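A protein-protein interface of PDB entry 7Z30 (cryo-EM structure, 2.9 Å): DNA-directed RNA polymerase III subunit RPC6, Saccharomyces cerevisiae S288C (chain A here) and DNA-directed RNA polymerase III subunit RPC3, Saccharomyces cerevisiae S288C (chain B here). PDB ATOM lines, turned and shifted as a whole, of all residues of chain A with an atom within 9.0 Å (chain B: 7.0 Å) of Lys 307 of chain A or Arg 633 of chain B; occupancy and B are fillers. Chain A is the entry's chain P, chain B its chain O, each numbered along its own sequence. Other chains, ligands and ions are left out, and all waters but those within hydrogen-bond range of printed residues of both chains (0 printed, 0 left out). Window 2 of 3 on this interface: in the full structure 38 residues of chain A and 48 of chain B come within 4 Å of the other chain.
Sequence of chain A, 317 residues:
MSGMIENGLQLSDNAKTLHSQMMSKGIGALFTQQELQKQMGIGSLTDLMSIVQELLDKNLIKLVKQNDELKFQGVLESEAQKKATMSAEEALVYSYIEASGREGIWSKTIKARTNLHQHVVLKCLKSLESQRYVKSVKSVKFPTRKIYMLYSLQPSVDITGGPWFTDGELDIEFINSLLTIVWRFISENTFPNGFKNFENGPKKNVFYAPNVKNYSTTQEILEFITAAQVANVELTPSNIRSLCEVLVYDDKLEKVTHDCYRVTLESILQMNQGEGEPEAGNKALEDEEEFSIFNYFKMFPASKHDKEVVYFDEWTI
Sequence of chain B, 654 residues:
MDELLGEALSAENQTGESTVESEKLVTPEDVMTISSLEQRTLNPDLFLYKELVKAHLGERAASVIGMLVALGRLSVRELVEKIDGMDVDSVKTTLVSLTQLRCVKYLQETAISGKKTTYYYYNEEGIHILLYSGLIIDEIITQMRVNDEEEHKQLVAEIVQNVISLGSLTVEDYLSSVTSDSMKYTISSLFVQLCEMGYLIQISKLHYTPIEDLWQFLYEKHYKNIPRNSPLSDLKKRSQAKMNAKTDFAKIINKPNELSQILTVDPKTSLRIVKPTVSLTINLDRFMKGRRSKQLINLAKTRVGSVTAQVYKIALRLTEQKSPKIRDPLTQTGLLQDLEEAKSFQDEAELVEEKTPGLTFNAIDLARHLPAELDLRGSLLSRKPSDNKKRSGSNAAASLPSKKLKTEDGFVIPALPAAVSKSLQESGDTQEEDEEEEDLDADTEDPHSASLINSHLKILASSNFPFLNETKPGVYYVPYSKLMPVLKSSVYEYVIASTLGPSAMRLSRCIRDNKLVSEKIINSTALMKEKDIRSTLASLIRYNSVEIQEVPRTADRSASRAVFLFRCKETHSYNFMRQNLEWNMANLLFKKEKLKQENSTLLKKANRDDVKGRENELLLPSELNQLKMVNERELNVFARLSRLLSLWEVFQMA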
ATOM      1  N   ALA A 302      19.894   2.711   7.049  1.00  0.00           N
ATOM      2  CA  ALA A 302      19.846   2.220   8.423  1.00  0.00           C
ATOM      3  C   ALA A 302      21.057   1.353   8.739  1.00  0.00           C
ATOM      4  O   ALA A 302      21.597   1.410   9.850  1.00  0.00           O
ATOM      5  CB  ALA A 302      18.550   1.445   8.658  1.00  0.00           C
ATOM      6  N   LYS A 304      21.543  -1.719   9.362  1.00  0.00           N
ATOM      7  CA  LYS A 304      21.363  -2.574  10.526  1.00  0.00           C
ATOM      8  C   LYS A 304      20.279  -3.594  10.214  1.00  0.00           C
ATOM      9  O   LYS A 304      19.428  -3.378   9.347  1.00  0.00           O
ATOM     10  CB  LYS A 304      21.002  -1.748  11.767  1.00  0.00           C
ATOM     11  CG  LYS A 304      21.131  -2.490  13.088  1.00  0.00           C
ATOM     12  CD  LYS A 304      21.077  -1.527  14.264  1.00  0.00           C
ATOM     13  CE  LYS A 304      22.450  -0.936  14.553  1.00  0.00           C
ATOM     14  NZ  LYS A 304      22.440  -0.038  15.741  1.00  0.00           N
ATOM     15  N   HIS A 305      20.321  -4.714  10.935  1.00  0.00           N
ATOM     16  CA  HIS A 305      19.295  -5.747  10.798  1.00  0.00           C
ATOM     17  C   HIS A 305      18.018  -5.405  11.548  1.00  0.00           C
ATOM     18  O   HIS A 305      17.183  -6.291  11.778  1.00  0.00           O
ATOM     19  CB  HIS A 305      19.841  -7.100  11.269  1.00  0.00           C
ATOM     20  CG  HIS A 305      19.927  -7.239  12.760  1.00  0.00           C
ATOM     21  ND1 HIS A 305      18.827  -7.486  13.553  1.00  0.00           N
ATOM     22  CD2 HIS A 305      20.988  -7.179  13.599  1.00  0.00           C
ATOM     23  CE1 HIS A 305      19.204  -7.564  14.816  1.00  0.00           C
ATOM     24  NE2 HIS A 305      20.512  -7.382  14.871  1.00  0.00           N
ATOM     25  N   ASP A 306      17.857  -4.141  11.930  1.00  0.00           N
ATOM     26  CA  ASP A 306      16.702  -3.706  12.697  1.00  0.00           C
ATOM     27  C   ASP A 306      15.441  -3.756  11.836  1.00  0.00           C
ATOM     28  O   ASP A 306      15.461  -4.131  10.660  1.00  0.00           O
ATOM     29  CB  ASP A 306      16.930  -2.299  13.245  1.00  0.00           C
ATOM     30  CG  ASP A 306      17.293  -1.301  12.159  1.00  0.00           C
ATOM     31  OD1 ASP A 306      17.563  -1.729  11.016  1.00  0.00           O
ATOM     32  OD2 ASP A 306      17.309  -0.085  12.448  1.00  0.00           O
ATOM     33  N   LYS A 307      14.328  -3.362  12.439  1.00  0.00           N
ATOM     34  CA  LYS A 307      13.032  -3.319  11.785  1.00  0.00           C
ATOM     35  C   LYS A 307      12.666  -1.866  11.504  1.00  0.00           C
ATOM     36  O   LYS A 307      13.483  -0.954  11.681  1.00  0.00           O
ATOM     37  CB  LYS A 307      11.979  -4.016  12.649  1.00  0.00           C
ATOM     38  CG  LYS A 307      11.928  -5.523  12.478  1.00  0.00           C
ATOM     39  CD  LYS A 307      12.861  -6.212  13.459  1.00  0.00           C
ATOM     40  CE  LYS A 307      12.382  -6.028  14.891  1.00  0.00           C
ATOM     41  NZ  LYS A 307      13.306  -6.662  15.870  1.00  0.00           N
ATOM     42  N   GLU A 308      11.436  -1.656  11.034  1.00  0.00           N
ATOM     43  CA  GLU A 308      10.872  -0.347  10.721  1.00  0.00           C
ATOM     44  C   GLU A 308      11.543   0.308   9.521  1.00  0.00           C
ATOM     45  O   GLU A 308      11.334   1.505   9.281  1.00  0.00           O
ATOM     46  CB  GLU A 308      10.937   0.605  11.922  1.00  0.00           C
ATOM     47  CG  GLU A 308      10.055   0.213  13.103  1.00  0.00           C
ATOM     48  CD  GLU A 308      10.652  -0.893  13.952  1.00  0.00           C
ATOM     49  OE1 GLU A 308      11.751  -0.691  14.509  1.00  0.00           O
ATOM     50  OE2 GLU A 308      10.015  -1.960  14.073  1.00  0.00           O
ATOM     51  N   VAL A 309      12.344  -0.438   8.761  1.00  0.00           N
ATOM     52  CA  VAL A 309      13.022   0.124   7.600  1.00  0.00           C
ATOM     53  C   VAL A 309      12.012   0.341   6.482  1.00  0.00           C
ATOM     54  O   VAL A 309      11.059  -0.434   6.324  1.00  0.00           O
ATOM     55  CB  VAL A 309      14.167  -0.798   7.149  1.00  0.00           C
ATOM     56  CG1 VAL A 309      15.017  -0.120   6.080  1.00  0.00           C
ATOM     57  CG2 VAL A 309      15.020  -1.210   8.340  1.00  0.00           C
ATOM     58  N   VAL A 310      12.211   1.401   5.706  1.00  0.00           N
ATOM     59  CA  VAL A 310      11.315   1.762   4.615  1.00  0.00           C
ATOM     60  C   VAL A 310      11.998   1.458   3.292  1.00  0.00           C
ATOM     61  O   VAL A 310      13.209   1.646   3.131  1.00  0.00           O
ATOM     62  CB  VAL A 310      10.903   3.245   4.701  1.00  0.00           C
ATOM     63  CG1 VAL A 310       9.662   3.508   3.860  1.00  0.00           C
ATOM     64  CG2 VAL A 310      10.681   3.645   6.147  1.00  0.00           C
ATOM     65  N   TYR A 311      11.210   0.979   2.332  1.00  0.00           N
ATOM     66  CA  TYR A 311      11.706   0.670   0.998  1.00  0.00           C
ATOM     67  C   TYR A 311      10.710   1.204  -0.016  1.00  0.00           C
ATOM     68  O   TYR A 311       9.497   1.083   0.176  1.00  0.00           O
ATOM     69  CB  TYR A 311      11.926  -0.839   0.795  1.00  0.00           C
ATOM     70  CG  TYR A 311      12.492  -1.577   1.997  1.00  0.00           C
ATOM     71  CD1 TYR A 311      11.723  -1.809   3.132  1.00  0.00           C
ATOM     72  CD2 TYR A 311      13.805  -2.029   1.996  1.00  0.00           C
ATOM     73  CE1 TYR A 311      12.241  -2.472   4.224  1.00  0.00           C
ATOM     74  CE2 TYR A 311      14.332  -2.695   3.086  1.00  0.00           C
ATOM     75  CZ  TYR A 311      13.545  -2.912   4.198  1.00  0.00           C
ATOM     76  OH  TYR A 311      14.061  -3.575   5.286  1.00  0.00           O
ATOM     77  N   ILE B  34       6.144 -11.751   8.539  1.00  0.00           N
ATOM     78  CA  ILE B  34       7.279 -10.837   8.518  1.00  0.00           C
ATOM     79  C   ILE B  34       7.458 -10.168   7.157  1.00  0.00           C
ATOM     80  O   ILE B  34       8.366  -9.337   7.002  1.00  0.00           O
ATOM     81  CB  ILE B  34       8.572 -11.571   8.940  1.00  0.00           C
ATOM     82  CG1 ILE B  34       9.511 -10.624   9.689  1.00  0.00           C
ATOM     83  CG2 ILE B  34       9.253 -12.227   7.740  1.00  0.00           C
ATOM     84  CD1 ILE B  34       9.070 -10.329  11.106  1.00  0.00           C
ATOM     85  N   LYS B 591       3.558  -0.510  12.198  1.00  0.00           N
ATOM     86  CA  LYS B 591       4.683  -1.055  12.949  1.00  0.00           C
ATOM     87  C   LYS B 591       4.701  -0.520  14.374  1.00  0.00           C
ATOM     88  O   LYS B 591       4.848  -1.289  15.332  1.00  0.00           O
ATOM     89  CB  LYS B 591       5.999  -0.722  12.245  1.00  0.00           C
ATOM     90  CG  LYS B 591       6.180  -1.365  10.878  1.00  0.00           C
ATOM     91  CD  LYS B 591       7.416  -2.244  10.831  1.00  0.00           C
ATOM     92  CE  LYS B 591       7.385  -3.170   9.628  1.00  0.00           C
ATOM     93  NZ  LYS B 591       8.662  -3.917   9.469  1.00  0.00           N
ATOM     94  N   LEU B 595       4.024  -2.678  17.767  1.00  0.00           N
ATOM     95  CA  LEU B 595       4.990  -2.690  18.861  1.00  0.00           C
ATOM     96  C   LEU B 595       4.323  -2.267  20.164  1.00  0.00           C
ATOM     97  O   LEU B 595       4.583  -2.846  21.223  1.00  0.00           O
ATOM     98  CB  LEU B 595       6.176  -1.782  18.519  1.00  0.00           C
ATOM     99  CG  LEU B 595       7.299  -1.491  19.527  1.00  0.00           C
ATOM    100  CD1 LEU B 595       6.960  -0.337  20.470  1.00  0.00           C
ATOM    101  CD2 LEU B 595       7.686  -2.742  20.311  1.00  0.00           C
ATOM    102  N   LEU B 627      13.132  -2.155  28.156  1.00  0.00           N
ATOM    103  CA  LEU B 627      12.410  -0.895  28.037  1.00  0.00           C
ATOM    104  C   LEU B 627      13.239   0.143  27.297  1.00  0.00           C
ATOM    105  O   LEU B 627      12.711   0.877  26.457  1.00  0.00           O
ATOM    106  CB  LEU B 627      12.001  -0.374  29.416  1.00  0.00           C
ATOM    107  CG  LEU B 627      10.560  -0.631  29.874  1.00  0.00           C
ATOM    108  CD1 LEU B 627       9.565   0.000  28.910  1.00  0.00           C
ATOM    109  CD2 LEU B 627      10.274  -2.108  30.038  1.00  0.00           C
ATOM    110  N   LYS B 628      14.536   0.232  27.601  1.00  0.00           N
ATOM    111  CA  LYS B 628      15.379   1.167  26.858  1.00  0.00           C
ATOM    112  C   LYS B 628      15.437   0.796  25.380  1.00  0.00           C
ATOM    113  O   LYS B 628      15.369   1.673  24.508  1.00  0.00           O
ATOM    114  CB  LYS B 628      16.790   1.249  27.448  1.00  0.00           C
ATOM    115  CG  LYS B 628      16.870   1.812  28.858  1.00  0.00           C
ATOM    116  CD  LYS B 628      17.528   0.846  29.828  1.00  0.00           C
ATOM    117  CE  LYS B 628      18.805   0.259  29.242  1.00  0.00           C
ATOM    118  NZ  LYS B 628      19.671  -0.328  30.303  1.00  0.00           N
ATOM    119  N   MET B 629      15.550  -0.504  25.073  1.00  0.00           N
ATOM    120  CA  MET B 629      15.597  -0.904  23.665  1.00  0.00           C
ATOM    121  C   MET B 629      14.309  -0.542  22.937  1.00  0.00           C
ATOM    122  O   MET B 629      14.353  -0.009  21.823  1.00  0.00           O
ATOM    123  CB  MET B 629      15.863  -2.402  23.500  1.00  0.00           C
ATOM    124  CG  MET B 629      16.921  -3.015  24.391  1.00  0.00           C
ATOM    125  SD  MET B 629      16.878  -4.810  24.201  1.00  0.00           S
ATOM    126  CE  MET B 629      17.422  -5.365  25.811  1.00  0.00           C
ATOM    127  N   VAL B 630      13.155  -0.831  23.541  1.00  0.00           N
ATOM    128  CA  VAL B 630      11.893  -0.544  22.865  1.00  0.00           C
ATOM    129  C   VAL B 630      11.648   0.962  22.781  1.00  0.00           C
ATOM    130  O   VAL B 630      11.102   1.451  21.783  1.00  0.00           O
ATOM    131  CB  VAL B 630      10.730  -1.293  23.547  1.00  0.00           C
ATOM    132  CG1 VAL B 630      11.008  -2.790  23.562  1.00  0.00           C
ATOM    133  CG2 VAL B 630      10.483  -0.784  24.960  1.00  0.00           C
ATOM    134  N   ASN B 631      12.050   1.723  23.803  1.00  0.00           N
ATOM    135  CA  ASN B 631      11.921   3.174  23.744  1.00  0.00           C
ATOM    136  C   ASN B 631      12.767   3.758  22.621  1.00  0.00           C
ATOM    137  O   ASN B 631      12.300   4.623  21.870  1.00  0.00           O
ATOM    138  CB  ASN B 631      12.310   3.789  25.089  1.00  0.00           C
ATOM    139  CG  ASN B 631      12.623   5.269  24.986  1.00  0.00           C
ATOM    140  OD1 ASN B 631      11.867   6.037  24.389  1.00  0.00           O
ATOM    141  ND2 ASN B 631      13.744   5.678  25.566  1.00  0.00           N
ATOM    142  N   GLU B 632      14.014   3.297  22.481  1.00  0.00           N
ATOM    143  CA  GLU B 632      14.848   3.813  21.401  1.00  0.00           C
ATOM    144  C   GLU B 632      14.349   3.329  20.044  1.00  0.00           C
ATOM    145  O   GLU B 632      14.492   4.033  19.040  1.00  0.00           O
ATOM    146  CB  GLU B 632      16.316   3.434  21.624  1.00  0.00           C
ATOM    147  CG  GLU B 632      16.663   1.975  21.403  1.00  0.00           C
ATOM    148  CD  GLU B 632      17.458   1.748  20.133  1.00  0.00           C
ATOM    149  OE1 GLU B 632      18.056   2.719  19.622  1.00  0.00           O
ATOM    150  OE2 GLU B 632      17.495   0.597  19.651  1.00  0.00           O
ATOM    151  N   ARG B 633      13.743   2.140  19.991  1.00  0.00           N
ATOM    152  CA  ARG B 633      13.140   1.675  18.744  1.00  0.00           C
ATOM    153  C   ARG B 633      11.978   2.572  18.328  1.00  0.00           C
ATOM    154  O   ARG B 633      11.839   2.924  17.148  1.00  0.00           O
ATOM    155  CB  ARG B 633      12.681   0.225  18.898  1.00  0.00           C
ATOM    156  CG  ARG B 633      13.800  -0.793  18.726  1.00  0.00           C
ATOM    157  CD  ARG B 633      13.298  -2.228  18.827  1.00  0.00           C
ATOM    158  NE  ARG B 633      11.956  -2.402  18.283  1.00  0.00           N
ATOM    159  CZ  ARG B 633      11.682  -2.575  16.997  1.00  0.00           C
ATOM    160  NH1 ARG B 633      12.638  -2.592  16.083  1.00  0.00           N
ATOM    161  NH2 ARG B 633      10.417  -2.740  16.620  1.00  0.00           N
ATOM    162  N   GLU B 634      11.139   2.962  19.290  1.00  0.00           N
ATOM    163  CA  GLU B 634      10.065   3.905  18.993  1.00  0.00           C
ATOM    164  C   GLU B 634      10.616   5.271  18.603  1.00  0.00           C
ATOM    165  O   GLU B 634      10.063   5.934  17.719  1.00  0.00           O
ATOM    166  CB  GLU B 634       9.121   4.021  20.191  1.00  0.00           C
ATOM    167  CG  GLU B 634       8.211   5.237  20.158  1.00  0.00           C
ATOM    168  CD  GLU B 634       7.925   5.789  21.538  1.00  0.00           C
ATOM    169  OE1 GLU B 634       8.523   5.290  22.513  1.00  0.00           O
ATOM    170  OE2 GLU B 634       7.102   6.721  21.647  1.00  0.00           O
ATOM    171  N   LEU B 635      11.701   5.710  19.245  1.00  0.00           N
ATOM    172  CA  LEU B 635      12.340   6.960  18.839  1.00  0.00           C
ATOM    173  C   LEU B 635      12.836   6.885  17.400  1.00  0.00           C
ATOM    174  O   LEU B 635      12.693   7.845  16.634  1.00  0.00           O
ATOM    175  CB  LEU B 635      13.491   7.293  19.786  1.00  0.00           C
ATOM    176  CG  LEU B 635      13.247   8.443  20.762  1.00  0.00           C
ATOM    177  CD1 LEU B 635      12.303   8.014  21.870  1.00  0.00           C
ATOM    178  CD2 LEU B 635      14.563   8.937  21.339  1.00  0.00           C
ATOM    179  N   ASN B 636      13.429   5.752  17.018  1.00  0.00           N
ATOM    180  CA  ASN B 636      13.887   5.576  15.643  1.00  0.00           C
ATOM    181  C   ASN B 636      12.721   5.590  14.664  1.00  0.00           C
ATOM    182  O   ASN B 636      12.818   6.181  13.581  1.00  0.00           O
ATOM    183  CB  ASN B 636      14.677   4.273  15.513  1.00  0.00           C
ATOM    184  CG  ASN B 636      15.881   4.224  16.428  1.00  0.00           C
ATOM    185  OD1 ASN B 636      16.181   5.188  17.132  1.00  0.00           O
ATOM    186  ND2 ASN B 636      16.582   3.097  16.422  1.00  0.00           N
ATOM    187  N   VAL B 637      11.612   4.933  15.014  1.00  0.00           N
ATOM    188  CA  VAL B 637      10.466   4.927  14.110  1.00  0.00           C
ATOM    189  C   VAL B 637       9.872   6.327  13.989  1.00  0.00           C
ATOM    190  O   VAL B 637       9.417   6.727  12.913  1.00  0.00           O
ATOM    191  CB  VAL B 637       9.414   3.884  14.541  1.00  0.00           C
ATOM    192  CG1 VAL B 637       8.448   4.439  15.573  1.00  0.00           C
ATOM    193  CG2 VAL B 637       8.640   3.402  13.325  1.00  0.00           C
ATOM    194  N   PHE B 638       9.893   7.107  15.075  1.00  0.00           N
ATOM    195  CA  PHE B 638       9.414   8.484  14.993  1.00  0.00           C
ATOM    196  C   PHE B 638      10.343   9.345  14.148  1.00  0.00           C
ATOM    197  O   PHE B 638       9.882  10.218  13.404  1.00  0.00           O
ATOM    198  CB  PHE B 638       9.255   9.078  16.392  1.00  0.00           C
ATOM    199  CG  PHE B 638       7.903   8.844  16.999  1.00  0.00           C
ATOM    200  CD1 PHE B 638       6.755   9.245  16.335  1.00  0.00           C
ATOM    201  CD2 PHE B 638       7.778   8.238  18.237  1.00  0.00           C
ATOM    202  CE1 PHE B 638       5.507   9.036  16.891  1.00  0.00           C
ATOM    203  CE2 PHE B 638       6.533   8.028  18.797  1.00  0.00           C
ATOM    204  CZ  PHE B 638       5.398   8.430  18.126  1.00  0.00           C
ATOM    205  N   ALA B 639      11.654   9.124  14.259  1.00  0.00           N
ATOM    206  CA  ALA B 639      12.597   9.849  13.412  1.00  0.00           C
ATOM    207  C   ALA B 639      12.377   9.520  11.941  1.00  0.00           C
ATOM    208  O   ALA B 639      12.394  10.416  11.090  1.00  0.00           O
ATOM    209  CB  ALA B 639      14.031   9.527  13.828  1.00  0.00           C
ATOM    210  N   ARG B 640      12.166   8.239  11.627  1.00  0.00           N
ATOM    211  CA  ARG B 640      11.860   7.852  10.253  1.00  0.00           C
ATOM    212  C   ARG B 640      10.547   8.468   9.788  1.00  0.00           C
ATOM    213  O   ARG B 640      10.434   8.916   8.641  1.00  0.00           O
ATOM    214  CB  ARG B 640      11.811   6.329  10.130  1.00  0.00           C
ATOM    215  CG  ARG B 640      13.013   5.723   9.426  1.00  0.00           C
ATOM    216  CD  ARG B 640      14.039   5.223  10.419  1.00  0.00           C
ATOM    217  NE  ARG B 640      13.473   4.229  11.322  1.00  0.00           N
ATOM    218  CZ  ARG B 640      14.179   3.514  12.188  1.00  0.00           C
ATOM    219  NH1 ARG B 640      15.488   3.667  12.305  1.00  0.00           N
ATOM    220  NH2 ARG B 640      13.555   2.625  12.954  1.00  0.00           N
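Among the printed residues, pairs that only touch across the chains: Lys 307 of chain A with Arg 633 of chain B, Lys 307 of chain A with Arg 640 of chain B, Glu 308 of chain A with Lys 591 of chain B, Glu 308 of chain A with Val 637 of chain B and Glu 308 of chain A with Arg 640 of chain B.
Of chain B, only Arg 633 and Arg 640 come within 4 Å of Lys 307 of chain A.
Of the printed residues of chain B, Glu 308 of chain A touches Lys 591 (3.9 Å), Arg 633 (2.6 Å), Val 637 (3.5 Å) and Arg 640 (3.5 Å).
No residue of chain A comes within 4 Å of Glu 632 of chain B.
Of the printed residues of chain A, Val 637 of chain B touches Glu 308.
Of the printed residues of chain A, Arg 640 of chain B touches Lys 307 and Glu 308.
The nearest residue of chain A that does not touch Arg 633 of chain B is Asp 306 of chain A (5.2 Å).
The guanidinium group (NH1) of Arg 633 of chain B lies within salt-bridge range of the side-chain carboxylate (OE1) of Glu 308 of chain A (2.6 Å).
Along chain A the printed residues that touch a printed residue of chain B span positions 307 to 308.
Hydrophobic or aromatic side chains of chain B that line the printed part of chain A: Val 637.
Among the printed residues, Asp or Glu carboxylates within 4 Å of a Lys or Arg side-chain nitrogen of the other chain: Glu 308 of chain A with Arg 633 of chain B (2.6 Å).
NE of Arg 640 of chain B is in hydrogen-bond range of O of Asn 636 of chain B (3.1 Å).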
